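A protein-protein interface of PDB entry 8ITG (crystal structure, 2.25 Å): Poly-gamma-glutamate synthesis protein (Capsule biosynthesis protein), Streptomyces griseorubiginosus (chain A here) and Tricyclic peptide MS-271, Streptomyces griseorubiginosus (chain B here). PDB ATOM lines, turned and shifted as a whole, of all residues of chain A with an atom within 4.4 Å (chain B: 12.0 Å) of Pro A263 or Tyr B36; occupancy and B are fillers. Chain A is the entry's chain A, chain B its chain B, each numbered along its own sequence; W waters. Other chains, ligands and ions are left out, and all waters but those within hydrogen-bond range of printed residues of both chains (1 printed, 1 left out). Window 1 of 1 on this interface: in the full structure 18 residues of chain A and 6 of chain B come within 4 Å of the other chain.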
ATOM      1  N   HIS A 167     -18.307  14.788 -26.503  1.00  0.00           N
ATOM      2  CA  HIS A 167     -17.133  15.646 -26.411  1.00  0.00           C
ATOM      3  C   HIS A 167     -16.558  15.546 -25.007  1.00  0.00           C
ATOM      4  O   HIS A 167     -17.273  15.261 -24.045  1.00  0.00           O
ATOM      5  CB  HIS A 167     -17.475  17.101 -26.741  1.00  0.00           C
ATOM      6  CG  HIS A 167     -18.492  17.696 -25.818  1.00  0.00           C
ATOM      7  ND1 HIS A 167     -18.165  18.213 -24.582  1.00  0.00           N
ATOM      8  CD2 HIS A 167     -19.832  17.845 -25.948  1.00  0.00           C
ATOM      9  CE1 HIS A 167     -19.260  18.659 -23.991  1.00  0.00           C
ATOM     10  NE2 HIS A 167     -20.284  18.444 -24.798  1.00  0.00           N
ATOM     11  N   ALA A 169     -14.025  17.503 -22.033  1.00  0.00           N
ATOM     12  CA  ALA A 169     -13.426  18.733 -21.540  1.00  0.00           C
ATOM     13  C   ALA A 169     -12.160  18.398 -20.770  1.00  0.00           C
ATOM     14  O   ALA A 169     -12.131  17.437 -19.993  1.00  0.00           O
ATOM     15  CB  ALA A 169     -14.395  19.505 -20.644  1.00  0.00           C
ATOM     16  N   PHE A 228      -8.794  25.832 -20.558  1.00  0.00           N
ATOM     17  CA  PHE A 228      -9.947  24.951 -20.709  1.00  0.00           C
ATOM     18  C   PHE A 228     -10.124  24.653 -22.187  1.00  0.00           C
ATOM     19  O   PHE A 228     -10.240  25.579 -22.994  1.00  0.00           O
ATOM     20  CB  PHE A 228     -11.209  25.600 -20.131  1.00  0.00           C
ATOM     21  CG  PHE A 228     -12.405  24.693 -20.094  1.00  0.00           C
ATOM     22  CD1 PHE A 228     -13.254  24.600 -21.183  1.00  0.00           C
ATOM     23  CD2 PHE A 228     -12.689  23.944 -18.964  1.00  0.00           C
ATOM     24  CE1 PHE A 228     -14.362  23.772 -21.152  1.00  0.00           C
ATOM     25  CE2 PHE A 228     -13.797  23.111 -18.925  1.00  0.00           C
ATOM     26  CZ  PHE A 228     -14.634  23.026 -20.022  1.00  0.00           C
ATOM     27  N   THR A 230     -12.040  21.859 -25.171  1.00  0.00           N
ATOM     28  CA  THR A 230     -13.037  20.847 -25.481  1.00  0.00           C
ATOM     29  C   THR A 230     -12.728  20.249 -26.844  1.00  0.00           C
ATOM     30  O   THR A 230     -12.211  20.928 -27.736  1.00  0.00           O
ATOM     31  CB  THR A 230     -14.456  21.423 -25.474  1.00  0.00           C
ATOM     32  OG1 THR A 230     -14.519  22.561 -26.343  1.00  0.00           O
ATOM     33  CG2 THR A 230     -14.851  21.839 -24.064  1.00  0.00           C
ATOM     34  N   HIS A 261     -26.046  22.920 -25.947  1.00  0.00           N
ATOM     35  CA  HIS A 261     -26.147  23.906 -24.878  1.00  0.00           C
ATOM     36  C   HIS A 261     -24.788  24.395 -24.402  1.00  0.00           C
ATOM     37  O   HIS A 261     -24.723  25.420 -23.715  1.00  0.00           O
ATOM     38  CB  HIS A 261     -26.882  23.330 -23.668  1.00  0.00           C
ATOM     39  CG  HIS A 261     -28.340  23.085 -23.891  1.00  0.00           C
ATOM     40  ND1 HIS A 261     -29.322  23.821 -23.264  1.00  0.00           N
ATOM     41  CD2 HIS A 261     -28.984  22.171 -24.654  1.00  0.00           C
ATOM     42  CE1 HIS A 261     -30.509  23.376 -23.638  1.00  0.00           C
ATOM     43  NE2 HIS A 261     -30.332  22.374 -24.479  1.00  0.00           N
ATOM     44  N   GLU A 262     -23.718  23.687 -24.742  1.00  0.00           N
ATOM     45  CA  GLU A 262     -22.425  23.919 -24.114  1.00  0.00           C
ATOM     46  C   GLU A 262     -21.918  25.325 -24.425  1.00  0.00           C
ATOM     47  O   GLU A 262     -21.837  25.703 -25.601  1.00  0.00           O
ATOM     48  CB  GLU A 262     -21.402  22.885 -24.586  1.00  0.00           C
ATOM     49  CG  GLU A 262     -21.696  21.445 -24.175  1.00  0.00           C
ATOM     50  CD  GLU A 262     -22.934  20.881 -24.843  1.00  0.00           C
ATOM     51  OE1 GLU A 262     -23.814  20.365 -24.124  1.00  0.00           O
ATOM     52  OE2 GLU A 262     -23.034  20.972 -26.086  1.00  0.00           O
ATOM     53  N   PRO A 263     -21.574  26.119 -23.416  1.00  0.00           N
ATOM     54  CA  PRO A 263     -21.037  27.457 -23.664  1.00  0.00           C
ATOM     55  C   PRO A 263     -19.533  27.440 -23.895  1.00  0.00           C
ATOM     56  O   PRO A 263     -18.813  26.537 -23.462  1.00  0.00           O
ATOM     57  CB  PRO A 263     -21.377  28.204 -22.371  1.00  0.00           C
ATOM     58  CG  PRO A 263     -21.309  27.137 -21.322  1.00  0.00           C
ATOM     59  CD  PRO A 263     -21.804  25.871 -21.982  1.00  0.00           C
ATOM     60  N   GLY A 264     -19.067  28.468 -24.597  1.00  0.00           N
ATOM     61  CA  GLY A 264     -17.654  28.715 -24.739  1.00  0.00           C
ATOM     62  C   GLY A 264     -17.150  29.561 -23.590  1.00  0.00           C
ATOM     63  O   GLY A 264     -17.730  29.566 -22.501  1.00  0.00           O
ATOM     64  N   THR A 266     -17.558  32.550 -23.066  1.00  0.00           N
ATOM     65  CA  THR A 266     -18.678  33.407 -22.715  1.00  0.00           C
ATOM     66  C   THR A 266     -19.964  32.697 -23.106  1.00  0.00           C
ATOM     67  O   THR A 266     -19.952  31.808 -23.964  1.00  0.00           O
ATOM     68  CB  THR A 266     -18.585  34.763 -23.433  1.00  0.00           C
ATOM     69  OG1 THR A 266     -18.733  34.567 -24.845  1.00  0.00           O
ATOM     70  CG2 THR A 266     -17.240  35.423 -23.156  1.00  0.00           C
ATOM     71  N   PRO A 267     -21.093  33.056 -22.486  1.00  0.00           N
ATOM     72  CA  PRO A 267     -22.351  32.361 -22.814  1.00  0.00           C
ATOM     73  C   PRO A 267     -22.749  32.462 -24.277  1.00  0.00           C
ATOM     74  O   PRO A 267     -23.374  31.531 -24.802  1.00  0.00           O
ATOM     75  CB  PRO A 267     -23.377  33.052 -21.903  1.00  0.00           C
ATOM     76  CG  PRO A 267     -22.575  33.591 -20.769  1.00  0.00           C
ATOM     77  CD  PRO A 267     -21.257  33.993 -21.360  1.00  0.00           C
ATOM     78  N   THR A 269     -20.707  32.576 -26.884  1.00  0.00           N
ATOM     79  CA  THR A 269     -19.866  31.898 -27.853  1.00  0.00           C
ATOM     80  C   THR A 269     -20.081  30.391 -27.787  1.00  0.00           C
ATOM     81  O   THR A 269     -20.305  29.833 -26.708  1.00  0.00           O
ATOM     82  CB  THR A 269     -18.392  32.209 -27.607  1.00  0.00           C
ATOM     83  OG1 THR A 269     -18.113  32.143 -26.203  1.00  0.00           O
ATOM     84  CG2 THR A 269     -18.039  33.591 -28.143  1.00  0.00           C
ATOM     85  N   GLY A 271     -19.102  26.372 -27.937  1.00  0.00           N
ATOM     86  CA  GLY A 271     -17.952  25.577 -27.553  1.00  0.00           C
ATOM     87  C   GLY A 271     -17.013  25.380 -28.727  1.00  0.00           C
ATOM     88  O   GLY A 271     -17.436  25.288 -29.882  1.00  0.00           O
ATOM     89  N   PHE A 273     -15.357  22.845 -29.597  1.00  0.00           N
ATOM     90  CA  PHE A 273     -15.629  21.591 -30.292  1.00  0.00           C
ATOM     91  C   PHE A 273     -16.761  21.756 -31.301  1.00  0.00           C
ATOM     92  O   PHE A 273     -16.749  21.131 -32.369  1.00  0.00           O
ATOM     93  CB  PHE A 273     -15.966  20.490 -29.285  1.00  0.00           C
ATOM     94  CG  PHE A 273     -17.353  20.600 -28.701  1.00  0.00           C
ATOM     95  CD1 PHE A 273     -17.601  21.433 -27.622  1.00  0.00           C
ATOM     96  CD2 PHE A 273     -18.405  19.870 -29.232  1.00  0.00           C
ATOM     97  CE1 PHE A 273     -18.873  21.538 -27.085  1.00  0.00           C
ATOM     98  CE2 PHE A 273     -19.681  19.972 -28.700  1.00  0.00           C
ATOM     99  CZ  PHE A 273     -19.913  20.807 -27.624  1.00  0.00           C
ATOM    100  N   ARG A 298     -27.016  32.965 -31.073  1.00  0.00           N
ATOM    101  CA  ARG A 298     -25.569  33.073 -31.164  1.00  0.00           C
ATOM    102  C   ARG A 298     -25.208  33.605 -32.547  1.00  0.00           C
ATOM    103  O   ARG A 298     -26.074  33.824 -33.398  1.00  0.00           O
ATOM    104  CB  ARG A 298     -24.896  31.727 -30.878  1.00  0.00           C
ATOM    105  CG  ARG A 298     -24.841  31.375 -29.400  1.00  0.00           C
ATOM    106  CD  ARG A 298     -24.259  29.987 -29.178  1.00  0.00           C
ATOM    107  NE  ARG A 298     -23.964  29.735 -27.771  1.00  0.00           N
ATOM    108  CZ  ARG A 298     -23.731  28.528 -27.263  1.00  0.00           C
ATOM    109  NH1 ARG A 298     -23.768  27.456 -28.044  1.00  0.00           N
ATOM    110  NH2 ARG A 298     -23.466  28.392 -25.970  1.00  0.00           N
ATOM    111  N   GLY B  33     -26.016  15.123 -16.083  1.00  0.00           N
ATOM    112  CA  GLY B  33     -24.899  15.048 -17.008  1.00  0.00           C
ATOM    113  C   GLY B  33     -24.770  16.253 -17.920  1.00  0.00           C
ATOM    114  O   GLY B  33     -25.202  16.217 -19.070  1.00  0.00           O
ATOM    115  N   CYS B  34     -24.183  17.333 -17.403  1.00  0.00           N
ATOM    116  CA  CYS B  34     -23.893  18.487 -18.247  1.00  0.00           C
ATOM    117  C   CYS B  34     -22.575  19.162 -17.886  1.00  0.00           C
ATOM    118  O   CYS B  34     -22.166  20.079 -18.601  1.00  0.00           O
ATOM    119  CB  CYS B  34     -25.047  19.513 -18.190  1.00  0.00           C
ATOM    120  SG  CYS B  34     -25.468  20.227 -19.817  1.00  0.00           S
ATOM    121  N   GLY B  35     -21.893  18.743 -16.825  1.00  0.00           N
ATOM    122  CA  GLY B  35     -20.596  19.300 -16.505  1.00  0.00           C
ATOM    123  C   GLY B  35     -20.696  20.767 -16.157  1.00  0.00           C
ATOM    124  O   GLY B  35     -21.418  21.164 -15.236  1.00  0.00           O
ATOM    125  N   TYR B  36     -19.974  21.588 -16.913  1.00  0.00           N
ATOM    126  CA  TYR B  36     -19.975  23.034 -16.744  1.00  0.00           C
ATOM    127  C   TYR B  36     -21.318  23.634 -17.153  1.00  0.00           C
ATOM    128  O   TYR B  36     -21.382  24.728 -17.720  1.00  0.00           O
ATOM    129  CB  TYR B  36     -18.836  23.663 -17.556  1.00  0.00           C
ATOM    130  CG  TYR B  36     -18.765  23.193 -18.998  1.00  0.00           C
ATOM    131  CD1 TYR B  36     -18.250  21.940 -19.324  1.00  0.00           C
ATOM    132  CD2 TYR B  36     -19.199  24.007 -20.033  1.00  0.00           C
ATOM    133  CE1 TYR B  36     -18.187  21.508 -20.641  1.00  0.00           C
ATOM    134  CE2 TYR B  36     -19.135  23.588 -21.350  1.00  0.00           C
ATOM    135  CZ  TYR B  36     -18.628  22.338 -21.649  1.00  0.00           C
ATOM    136  OH  TYR B  36     -18.561  21.913 -22.957  1.00  0.00           O
ATOM    137  N   CYS B  40     -28.108  23.121 -18.186  1.00  0.00           N
ATOM    138  CA  CYS B  40     -28.521  23.225 -19.579  1.00  0.00           C
ATOM    139  C   CYS B  40     -30.035  23.023 -19.698  1.00  0.00           C
ATOM    140  O   CYS B  40     -30.519  21.919 -19.940  1.00  0.00           O
ATOM    141  CB  CYS B  40     -27.747  22.220 -20.446  1.00  0.00           C
ATOM    142  SG  CYS B  40     -27.482  20.545 -19.776  1.00  0.00           S
ATOM    143  N   PHE B  41     -30.767  24.122 -19.536  1.00  0.00           N
ATOM    144  CA  PHE B  41     -32.207  24.092 -19.321  1.00  0.00           C
ATOM    145  C   PHE B  41     -32.968  23.962 -20.636  1.00  0.00           C
ATOM    146  O   PHE B  41     -32.511  24.411 -21.690  1.00  0.00           O
ATOM    147  CB  PHE B  41     -32.636  25.371 -18.598  1.00  0.00           C
ATOM    148  CG  PHE B  41     -33.717  25.177 -17.568  1.00  0.00           C
ATOM    149  CD1 PHE B  41     -33.397  25.106 -16.223  1.00  0.00           C
ATOM    150  CD2 PHE B  41     -35.051  25.100 -17.940  1.00  0.00           C
ATOM    151  CE1 PHE B  41     -34.384  24.945 -15.266  1.00  0.00           C
ATOM    152  CE2 PHE B  41     -36.048  24.939 -16.986  1.00  0.00           C
ATOM    153  CZ  PHE B  41     -35.713  24.860 -15.647  1.00  0.00           C
HETATM  154  O   HOH W   1     -16.804  19.670 -22.758  1.00  0.00           O
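The side-chain hydroxyl (OG1) of Thr A230 lies within hydrogen-bond range of the backbone NH (N) of Phe A273 (3.4 Å). The backbone carbonyl oxygen (O) of Glu A262 lies within hydrogen-bond range of the guanidinium group (NH2) of Arg A298, 3.2 Å away. The side-chain sulfur (SG) of Cys B34 forms a disulfide with the side-chain sulfur (SG) of Cys B40 (2.0 Å).
Among the printed residues, merely in contact across the chains: His A167 with Tyr B36 (3.5 Å), Phe A228 with Tyr B36 (3.8 Å), Thr A230 with Tyr B36 (3.9 Å), His A261 with Cys B40 (3.5 Å), His A261 with Phe B41 (3.0 Å), Glu A262 with Tyr B36 (3.4 Å) and Pro A263 with Tyr B36 (3.6 Å).
Hydrophobic or aromatic side chains of chain B that line the printed part of chain A: Tyr B36. Hydrophobic or aromatic side chains of chain A that line the printed part of chain B: His A167, Phe A228, His A261 and Pro A263. Among the printed residues, 7 pairs touch across the chains. Among the printed residues, no Asp or Glu carboxylate lies within 4 Å of a Lys or Arg side-chain nitrogen of the other chain.
Of chain B, only Tyr B36 (3.6 Å) comes within 4 Å of Pro A263. Printed residues of chain A within 4 Å of Tyr B36: His A167 (3.5 Å), Phe A228 (3.8 Å), Thr A230 (3.9 Å), Glu A262 (3.4 Å) and Pro A263 (3.6 Å). No residue of chain B comes within 4 Å of Ala A169. Glu A262 touches one residue of chain B. No residue of chain B comes within 4 Å of Gly A264. Printed residues of chain B within 4 Å of His A261: Cys B40 and Phe B41. Of the printed residues of chain B, Phe A228 touches Tyr B36. Of the printed residues of chain A, Phe B41 touches His A261. Of the printed residues of chain A, Cys B40 touches His A261 (3.5 Å). Of the printed residues of chain B, Thr A230 touches Tyr B36 (3.9 Å). The nearest residue of chain A that does not touch Tyr B36 is Phe A273 (4.2 Å).
Water W1 bridges a ring nitrogen (ND1) of His A167 (2.7 Å) and the side-chain hydroxyl of Tyr B36 (2.9 Å).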
